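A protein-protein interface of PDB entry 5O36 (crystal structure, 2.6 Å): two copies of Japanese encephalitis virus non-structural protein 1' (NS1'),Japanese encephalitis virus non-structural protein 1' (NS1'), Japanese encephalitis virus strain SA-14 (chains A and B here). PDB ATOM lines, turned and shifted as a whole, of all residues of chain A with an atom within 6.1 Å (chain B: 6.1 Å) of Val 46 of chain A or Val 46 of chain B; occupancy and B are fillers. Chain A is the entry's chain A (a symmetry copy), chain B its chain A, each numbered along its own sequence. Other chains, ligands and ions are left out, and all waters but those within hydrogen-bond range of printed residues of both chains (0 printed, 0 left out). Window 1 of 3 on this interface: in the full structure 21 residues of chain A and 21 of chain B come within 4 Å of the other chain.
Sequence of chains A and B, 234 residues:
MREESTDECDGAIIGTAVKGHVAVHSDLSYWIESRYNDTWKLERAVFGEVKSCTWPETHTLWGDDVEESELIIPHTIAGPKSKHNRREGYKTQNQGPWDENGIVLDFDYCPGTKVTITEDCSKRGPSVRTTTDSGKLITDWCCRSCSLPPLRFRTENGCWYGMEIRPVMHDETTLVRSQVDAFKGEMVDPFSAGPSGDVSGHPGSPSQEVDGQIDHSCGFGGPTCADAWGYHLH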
ATOM      1  N   SER A  29      26.289 -29.412   1.932  1.00  0.00           N
ATOM      2  CA  SER A  29      27.381 -28.898   2.790  1.00  0.00           C
ATOM      3  C   SER A  29      27.366 -27.413   3.094  1.00  0.00           C
ATOM      4  O   SER A  29      27.883 -27.033   4.142  1.00  0.00           O
ATOM      5  CB  SER A  29      28.775 -29.287   2.283  1.00  0.00           C
ATOM      6  OG  SER A  29      28.870 -29.136   0.894  1.00  0.00           O
ATOM      7  N   TYR A  30      26.784 -26.577   2.224  1.00  0.00           N
ATOM      8  CA  TYR A  30      26.858 -25.113   2.376  1.00  0.00           C
ATOM      9  C   TYR A  30      25.545 -24.544   2.892  1.00  0.00           C
ATOM     10  O   TYR A  30      24.476 -25.074   2.584  1.00  0.00           O
ATOM     11  CB  TYR A  30      27.133 -24.496   1.033  1.00  0.00           C
ATOM     12  CG  TYR A  30      28.512 -24.671   0.476  1.00  0.00           C
ATOM     13  CD1 TYR A  30      29.439 -25.600   1.007  1.00  0.00           C
ATOM     14  CD2 TYR A  30      28.904 -23.904  -0.617  1.00  0.00           C
ATOM     15  CE1 TYR A  30      30.718 -25.729   0.464  1.00  0.00           C
ATOM     16  CE2 TYR A  30      30.172 -24.027  -1.173  1.00  0.00           C
ATOM     17  CZ  TYR A  30      31.075 -24.935  -0.613  1.00  0.00           C
ATOM     18  OH  TYR A  30      32.292 -25.067  -1.145  1.00  0.00           O
ATOM     19  N   TRP A  31      25.616 -23.486   3.692  1.00  0.00           N
ATOM     20  CA  TRP A  31      24.426 -22.722   4.105  1.00  0.00           C
ATOM     21  C   TRP A  31      24.869 -21.279   4.031  1.00  0.00           C
ATOM     22  O   TRP A  31      25.742 -20.861   4.785  1.00  0.00           O
ATOM     23  CB  TRP A  31      23.973 -23.076   5.528  1.00  0.00           C
ATOM     24  CG  TRP A  31      23.165 -22.023   6.226  1.00  0.00           C
ATOM     25  CD1 TRP A  31      23.621 -20.846   6.885  1.00  0.00           C
ATOM     26  CD2 TRP A  31      21.772 -22.015   6.367  1.00  0.00           C
ATOM     27  NE1 TRP A  31      22.550 -20.133   7.425  1.00  0.00           N
ATOM     28  CE2 TRP A  31      21.409 -20.826   7.101  1.00  0.00           C
ATOM     29  CE3 TRP A  31      20.799 -22.879   5.970  1.00  0.00           C
ATOM     30  CZ2 TRP A  31      20.133 -20.527   7.404  1.00  0.00           C
ATOM     31  CZ3 TRP A  31      19.504 -22.582   6.269  1.00  0.00           C
ATOM     32  CH2 TRP A  31      19.171 -21.407   6.967  1.00  0.00           C
ATOM     33  N   ILE A  32      24.300 -20.534   3.101  1.00  0.00           N
ATOM     34  CA  ILE A  32      24.755 -19.177   2.818  1.00  0.00           C
ATOM     35  C   ILE A  32      23.593 -18.202   2.991  1.00  0.00           C
ATOM     36  O   ILE A  32      22.617 -18.315   2.280  1.00  0.00           O
ATOM     37  CB  ILE A  32      25.303 -19.117   1.404  1.00  0.00           C
ATOM     38  CG1 ILE A  32      26.494 -20.106   1.265  1.00  0.00           C
ATOM     39  CG2 ILE A  32      25.689 -17.702   1.055  1.00  0.00           C
ATOM     40  CD1 ILE A  32      26.936 -20.332  -0.167  1.00  0.00           C
ATOM     41  N   ARG A  44      26.306 -14.385   6.603  1.00  0.00           N
ATOM     42  CA  ARG A  44      27.131 -15.470   7.118  1.00  0.00           C
ATOM     43  C   ARG A  44      27.014 -16.695   6.230  1.00  0.00           C
ATOM     44  O   ARG A  44      26.036 -16.850   5.502  1.00  0.00           O
ATOM     45  CB  ARG A  44      26.796 -15.805   8.584  1.00  0.00           C
ATOM     46  CG  ARG A  44      25.679 -16.783   8.747  1.00  0.00           C
ATOM     47  CD  ARG A  44      25.403 -17.087  10.204  1.00  0.00           C
ATOM     48  NE  ARG A  44      24.236 -16.338  10.644  1.00  0.00           N
ATOM     49  CZ  ARG A  44      24.256 -15.232  11.386  1.00  0.00           C
ATOM     50  NH1 ARG A  44      25.394 -14.683  11.846  1.00  0.00           N
ATOM     51  NH2 ARG A  44      23.099 -14.644  11.667  1.00  0.00           N
ATOM     52  N   ALA A  45      28.036 -17.536   6.282  1.00  0.00           N
ATOM     53  CA  ALA A  45      28.054 -18.736   5.493  1.00  0.00           C
ATOM     54  C   ALA A  45      28.705 -19.831   6.321  1.00  0.00           C
ATOM     55  O   ALA A  45      29.697 -19.579   7.005  1.00  0.00           O
ATOM     56  CB  ALA A  45      28.797 -18.489   4.186  1.00  0.00           C
ATOM     57  N   VAL A  46      28.124 -21.035   6.276  1.00  0.00           N
ATOM     58  CA  VAL A  46      28.573 -22.178   7.083  1.00  0.00           C
ATOM     59  C   VAL A  46      28.891 -23.323   6.152  1.00  0.00           C
ATOM     60  O   VAL A  46      28.170 -23.545   5.187  1.00  0.00           O
ATOM     61  CB  VAL A  46      27.483 -22.533   8.078  1.00  0.00           C
ATOM     62  CG1 VAL A  46      27.972 -23.483   9.104  1.00  0.00           C
ATOM     63  CG2 VAL A  46      27.033 -21.252   8.801  1.00  0.00           C
ATOM     64  N   PHE A  47      29.994 -24.019   6.405  1.00  0.00           N
ATOM     65  CA  PHE A  47      30.546 -24.988   5.451  1.00  0.00           C
ATOM     66  C   PHE A  47      30.923 -26.265   6.134  1.00  0.00           C
ATOM     67  O   PHE A  47      31.815 -26.264   6.999  1.00  0.00           O
ATOM     68  CB  PHE A  47      31.806 -24.470   4.756  1.00  0.00           C
ATOM     69  CG  PHE A  47      31.630 -23.165   4.053  1.00  0.00           C
ATOM     70  CD1 PHE A  47      31.763 -21.968   4.744  1.00  0.00           C
ATOM     71  CD2 PHE A  47      31.339 -23.129   2.700  1.00  0.00           C
ATOM     72  CE1 PHE A  47      31.582 -20.760   4.100  1.00  0.00           C
ATOM     73  CE2 PHE A  47      31.181 -21.926   2.042  1.00  0.00           C
ATOM     74  CZ  PHE A  47      31.310 -20.735   2.742  1.00  0.00           C
ATOM     75  N   GLY A  48      30.266 -27.354   5.753  1.00  0.00           N
ATOM     76  CA  GLY A  48      30.626 -28.671   6.229  1.00  0.00           C
ATOM     77  C   GLY A  48      31.961 -29.031   5.622  1.00  0.00           C
ATOM     78  O   GLY A  48      32.943 -29.221   6.308  1.00  0.00           O
ATOM     79  N   GLY A 102      34.607 -27.649   8.475  1.00  0.00           N
ATOM     80  CA  GLY A 102      33.747 -26.901   9.440  1.00  0.00           C
ATOM     81  C   GLY A 102      33.908 -25.361   9.595  1.00  0.00           C
ATOM     82  O   GLY A 102      33.670 -24.816  10.671  1.00  0.00           O
ATOM     83  N   ILE A 103      34.252 -24.669   8.519  1.00  0.00           N
ATOM     84  CA  ILE A 103      34.446 -23.219   8.491  1.00  0.00           C
ATOM     85  C   ILE A 103      33.139 -22.407   8.606  1.00  0.00           C
ATOM     86  O   ILE A 103      32.095 -22.775   8.025  1.00  0.00           O
ATOM     87  CB  ILE A 103      35.072 -22.845   7.140  1.00  0.00           C
ATOM     88  CG1 ILE A 103      36.454 -23.485   7.019  1.00  0.00           C
ATOM     89  CG2 ILE A 103      35.103 -21.333   6.880  1.00  0.00           C
ATOM     90  CD1 ILE A 103      36.889 -23.574   5.568  1.00  0.00           C
ATOM     91  N   VAL A 104      33.226 -21.287   9.337  1.00  0.00           N
ATOM     92  CA  VAL A 104      32.180 -20.256   9.391  1.00  0.00           C
ATOM     93  C   VAL A 104      32.711 -18.924   8.897  1.00  0.00           C
ATOM     94  O   VAL A 104      33.771 -18.497   9.298  1.00  0.00           O
ATOM     95  CB  VAL A 104      31.677 -20.035  10.829  1.00  0.00           C
ATOM     96  CG1 VAL A 104      30.489 -19.079  10.833  1.00  0.00           C
ATOM     97  CG2 VAL A 104      31.308 -21.367  11.461  1.00  0.00           C
ATOM     98  N   LEU A 105      31.947 -18.263   8.043  1.00  0.00           N
ATOM     99  CA  LEU A 105      32.290 -16.952   7.508  1.00  0.00           C
ATOM    100  C   LEU A 105      31.232 -15.972   7.948  1.00  0.00           C
ATOM    101  O   LEU A 105      30.069 -16.166   7.675  1.00  0.00           O
ATOM    102  CB  LEU A 105      32.309 -17.021   5.984  1.00  0.00           C
ATOM    103  CG  LEU A 105      32.991 -15.898   5.197  1.00  0.00           C
ATOM    104  CD1 LEU A 105      32.939 -16.205   3.714  1.00  0.00           C
ATOM    105  CD2 LEU A 105      32.334 -14.572   5.419  1.00  0.00           C
ATOM    106  N   SER B  29      20.331 -27.778   6.406  1.00  0.00           N
ATOM    107  CA  SER B  29      21.019 -26.962   7.433  1.00  0.00           C
ATOM    108  C   SER B  29      22.091 -27.656   8.248  1.00  0.00           C
ATOM    109  O   SER B  29      23.000 -26.970   8.709  1.00  0.00           O
ATOM    110  CB  SER B  29      20.047 -26.256   8.387  1.00  0.00           C
ATOM    111  OG  SER B  29      19.009 -27.112   8.778  1.00  0.00           O
ATOM    112  N   TYR B  30      22.018 -28.982   8.424  1.00  0.00           N
ATOM    113  CA  TYR B  30      22.936 -29.704   9.322  1.00  0.00           C
ATOM    114  C   TYR B  30      23.994 -30.464   8.537  1.00  0.00           C
ATOM    115  O   TYR B  30      23.726 -30.933   7.429  1.00  0.00           O
ATOM    116  CB  TYR B  30      22.149 -30.704  10.124  1.00  0.00           C
ATOM    117  CG  TYR B  30      21.262 -30.162  11.201  1.00  0.00           C
ATOM    118  CD1 TYR B  30      20.928 -28.789  11.298  1.00  0.00           C
ATOM    119  CD2 TYR B  30      20.726 -31.036  12.143  1.00  0.00           C
ATOM    120  CE1 TYR B  30      20.102 -28.321  12.321  1.00  0.00           C
ATOM    121  CE2 TYR B  30      19.897 -30.585  13.163  1.00  0.00           C
ATOM    122  CZ  TYR B  30      19.604 -29.221  13.248  1.00  0.00           C
ATOM    123  OH  TYR B  30      18.801 -28.779  14.219  1.00  0.00           O
ATOM    124  N   TRP B  31      25.198 -30.568   9.087  1.00  0.00           N
ATOM    125  CA  TRP B  31      26.253 -31.433   8.531  1.00  0.00           C
ATOM    126  C   TRP B  31      26.887 -32.071   9.745  1.00  0.00           C
ATOM    127  O   TRP B  31      27.495 -31.382  10.559  1.00  0.00           O
ATOM    128  CB  TRP B  31      27.295 -30.640   7.731  1.00  0.00           C
ATOM    129  CG  TRP B  31      28.639 -31.291   7.600  1.00  0.00           C
ATOM    130  CD1 TRP B  31      29.701 -31.334   8.548  1.00  0.00           C
ATOM    131  CD2 TRP B  31      29.108 -31.990   6.482  1.00  0.00           C
ATOM    132  NE1 TRP B  31      30.797 -32.028   8.035  1.00  0.00           N
ATOM    133  CE2 TRP B  31      30.443 -32.451   6.777  1.00  0.00           C
ATOM    134  CE3 TRP B  31      28.559 -32.264   5.267  1.00  0.00           C
ATOM    135  CZ2 TRP B  31      31.173 -33.159   5.896  1.00  0.00           C
ATOM    136  CZ3 TRP B  31      29.290 -32.983   4.371  1.00  0.00           C
ATOM    137  CH2 TRP B  31      30.581 -33.441   4.688  1.00  0.00           C
ATOM    138  N   ILE B  32      26.712 -33.372   9.888  1.00  0.00           N
ATOM    139  CA  ILE B  32      27.130 -34.076  11.095  1.00  0.00           C
ATOM    140  C   ILE B  32      28.106 -35.191  10.725  1.00  0.00           C
ATOM    141  O   ILE B  32      27.729 -36.089  10.003  1.00  0.00           O
ATOM    142  CB  ILE B  32      25.908 -34.641  11.795  1.00  0.00           C
ATOM    143  CG1 ILE B  32      24.944 -33.482  12.175  1.00  0.00           C
ATOM    144  CG2 ILE B  32      26.324 -35.457  12.993  1.00  0.00           C
ATOM    145  CD1 ILE B  32      23.574 -33.950  12.624  1.00  0.00           C
ATOM    146  N   ARG B  44      32.402 -33.768  14.533  1.00  0.00           N
ATOM    147  CA  ARG B  44      31.994 -32.371  14.459  1.00  0.00           C
ATOM    148  C   ARG B  44      30.639 -32.248  13.789  1.00  0.00           C
ATOM    149  O   ARG B  44      30.225 -33.132  13.043  1.00  0.00           O
ATOM    150  CB  ARG B  44      33.051 -31.497  13.758  1.00  0.00           C
ATOM    151  CG  ARG B  44      32.917 -31.454  12.270  1.00  0.00           C
ATOM    152  CD  ARG B  44      33.968 -30.570  11.634  1.00  0.00           C
ATOM    153  NE  ARG B  44      35.030 -31.397  11.083  1.00  0.00           N
ATOM    154  CZ  ARG B  44      36.228 -31.593  11.631  1.00  0.00           C
ATOM    155  NH1 ARG B  44      36.609 -31.007  12.779  1.00  0.00           N
ATOM    156  NH2 ARG B  44      37.073 -32.415  11.018  1.00  0.00           N
ATOM    157  N   ALA B  45      29.951 -31.156  14.091  1.00  0.00           N
ATOM    158  CA  ALA B  45      28.653 -30.912  13.526  1.00  0.00           C
ATOM    159  C   ALA B  45      28.532 -29.422  13.258  1.00  0.00           C
ATOM    160  O   ALA B  45      28.961 -28.612  14.078  1.00  0.00           O
ATOM    161  CB  ALA B  45      27.570 -31.414  14.472  1.00  0.00           C
ATOM    162  N   VAL B  46      27.972 -29.071  12.095  1.00  0.00           N
ATOM    163  CA  VAL B  46      27.857 -27.678  11.642  1.00  0.00           C
ATOM    164  C   VAL B  46      26.402 -27.382  11.369  1.00  0.00           C
ATOM    165  O   VAL B  46      25.699 -28.225  10.826  1.00  0.00           O
ATOM    166  CB  VAL B  46      28.722 -27.491  10.409  1.00  0.00           C
ATOM    167  CG1 VAL B  46      28.879 -26.058  10.066  1.00  0.00           C
ATOM    168  CG2 VAL B  46      30.122 -28.062  10.691  1.00  0.00           C
ATOM    169  N   PHE B  47      25.935 -26.212  11.788  1.00  0.00           N
ATOM    170  CA  PHE B  47      24.500 -25.903  11.808  1.00  0.00           C
ATOM    171  C   PHE B  47      24.231 -24.545  11.240  1.00  0.00           C
ATOM    172  O   PHE B  47      24.689 -23.537  11.804  1.00  0.00           O
ATOM    173  CB  PHE B  47      23.920 -25.912  13.223  1.00  0.00           C
ATOM    174  CG  PHE B  47      24.137 -27.187  13.970  1.00  0.00           C
ATOM    175  CD1 PHE B  47      25.318 -27.402  14.669  1.00  0.00           C
ATOM    176  CD2 PHE B  47      23.162 -28.169  13.982  1.00  0.00           C
ATOM    177  CE1 PHE B  47      25.529 -28.587  15.345  1.00  0.00           C
ATOM    178  CE2 PHE B  47      23.353 -29.347  14.676  1.00  0.00           C
ATOM    179  CZ  PHE B  47      24.538 -29.556  15.366  1.00  0.00           C
ATOM    180  N   GLY B  48      23.489 -24.502  10.139  1.00  0.00           N
ATOM    181  CA  GLY B  48      23.039 -23.252   9.568  1.00  0.00           C
ATOM    182  C   GLY B  48      22.020 -22.656  10.510  1.00  0.00           C
ATOM    183  O   GLY B  48      22.207 -21.592  11.061  1.00  0.00           O
ATOM    184  N   GLY B 102      24.374 -20.299  12.951  1.00  0.00           N
ATOM    185  CA  GLY B 102      25.772 -20.646  12.555  1.00  0.00           C
ATOM    186  C   GLY B 102      26.713 -21.361  13.567  1.00  0.00           C
ATOM    187  O   GLY B 102      27.927 -21.177  13.524  1.00  0.00           O
ATOM    188  N   ILE B 103      26.162 -22.209  14.423  1.00  0.00           N
ATOM    189  CA  ILE B 103      26.899 -22.962  15.437  1.00  0.00           C
ATOM    190  C   ILE B 103      27.775 -24.097  14.866  1.00  0.00           C
ATOM    191  O   ILE B 103      27.375 -24.808  13.918  1.00  0.00           O
ATOM    192  CB  ILE B 103      25.882 -23.628  16.374  1.00  0.00           C
ATOM    193  CG1 ILE B 103      25.078 -22.556  17.108  1.00  0.00           C
ATOM    194  CG2 ILE B 103      26.512 -24.646  17.334  1.00  0.00           C
ATOM    195  CD1 ILE B 103      23.772 -23.119  17.636  1.00  0.00           C
ATOM    196  N   VAL B 104      28.955 -24.269  15.477  1.00  0.00           N
ATOM    197  CA  VAL B 104      29.838 -25.421  15.250  1.00  0.00           C
ATOM    198  C   VAL B 104      30.057 -26.194  16.537  1.00  0.00           C
ATOM    199  O   VAL B 104      30.343 -25.614  17.561  1.00  0.00           O
ATOM    200  CB  VAL B 104      31.226 -24.982  14.748  1.00  0.00           C
ATOM    201  CG1 VAL B 104      32.064 -26.200  14.374  1.00  0.00           C
ATOM    202  CG2 VAL B 104      31.075 -24.037  13.567  1.00  0.00           C
ATOM    203  N   LEU B 105      29.944 -27.509  16.464  1.00  0.00           N
ATOM    204  CA  LEU B 105      30.166 -28.399  17.597  1.00  0.00           C
ATOM    205  C   LEU B 105      31.330 -29.300  17.268  1.00  0.00           C
ATOM    206  O   LEU B 105      31.300 -29.997  16.279  1.00  0.00           O
ATOM    207  CB  LEU B 105      28.919 -29.248  17.820  1.00  0.00           C
ATOM    208  CG  LEU B 105      28.750 -29.987  19.151  1.00  0.00           C
ATOM    209  CD1 LEU B 105      27.420 -30.713  19.171  1.00  0.00           C
ATOM    210  CD2 LEU B 105      29.832 -30.995  19.379  1.00  0.00           C
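Among the printed residues, pairs that only touch across the chains: Val 46 of chain A with Val 46 of chain B (2.9 Å), Val 104 of chain A with Val 104 of chain B (3.4 Å), Gly 48 of chain A with Trp 31 of chain B (3.6 Å), Trp 31 of chain A with Gly 48 of chain B (3.6 Å), Val 104 of chain A with Gly 102 of chain B (3.97 Å) and Gly 102 of chain A with Val 104 of chain B (3.97 Å).
The backbone carbonyl oxygen (O) of Ser 29 of chain B lies within hydrogen-bond range of the backbone NH (N) of Gly 48 of chain B (2.9 Å).
The backbone carbonyl oxygen of Trp 31 of chain B lies within hydrogen-bond range of the backbone NH of Val 46 of chain B (2.8 Å).
N of Gly 102 of chain B lies close to O of Phe 47 of chain B.
N of Gly 102 of chain B lies within hydrogen-bond range of O of Gly 48 of chain B (3.2 Å).
The backbone carbonyl oxygen (O) of Trp 31 of chain A lies within hydrogen-bond range of the backbone NH (N) of Val 46 of chain A (2.8 Å).
O of Phe 47 of chain A lies close to N of Gly 102 of chain A (3.4 Å).
Trp 31 of chain A touches Gly 48 of chain B, and with the chains exchanged Gly 48 of chain A touches Trp 31 of chain B.
Val 46 of chain A touches its own counterpart, Val 46 of chain B.
Gly 102 of chain A touches Val 104 of chain B, and with the chains exchanged Val 104 of chain A touches Gly 102 of chain B.
Val 104 of chain A touches its own counterpart, Val 104 of chain B.
Positions printed for both chains: 29, 30, 31, 32, 44, 45, 46, 47, 48, 102, 103, 104 and 105.
Of the 6 pairs that touch across the chains among the printed residues, 6 have their exchanged pair printed and touching as well.
Printed residues of chain A that touch a printed residue of chain B: Trp 31, Val 46, Gly 48, Gly 102 and Val 104.
Hydrophobic or aromatic side chains of chain A within 4 Å of the printed part of chain B: Trp 31, Val 46 and Val 104.
Of the 13 printed residues of chain B, 5 touch a printed residue of chain A.
Printed residues of chain B that touch a printed residue of chain A: Trp 31, Val 46, Gly 48, Gly 102 and Val 104.
Of the printed residues of chain B, Trp 31 of chain A touches Gly 48.
Of the printed residues of chain B, Val 46 of chain A touches Val 46.
Printed residues of chain B within 4 Å of Gly 48 of chain A: Trp 31 (3.6 Å).
Printed residues of chain A within 4 Å of Trp 31 of chain B: Gly 48 (3.6 Å).
Of the printed residues of chain A, Val 46 of chain B touches Val 46.
Printed residues of chain A within 4 Å of Gly 48 of chain B: Trp 31.
Of the printed residues of chain A, Val 104 of chain B touches Gly 102 and Val 104.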
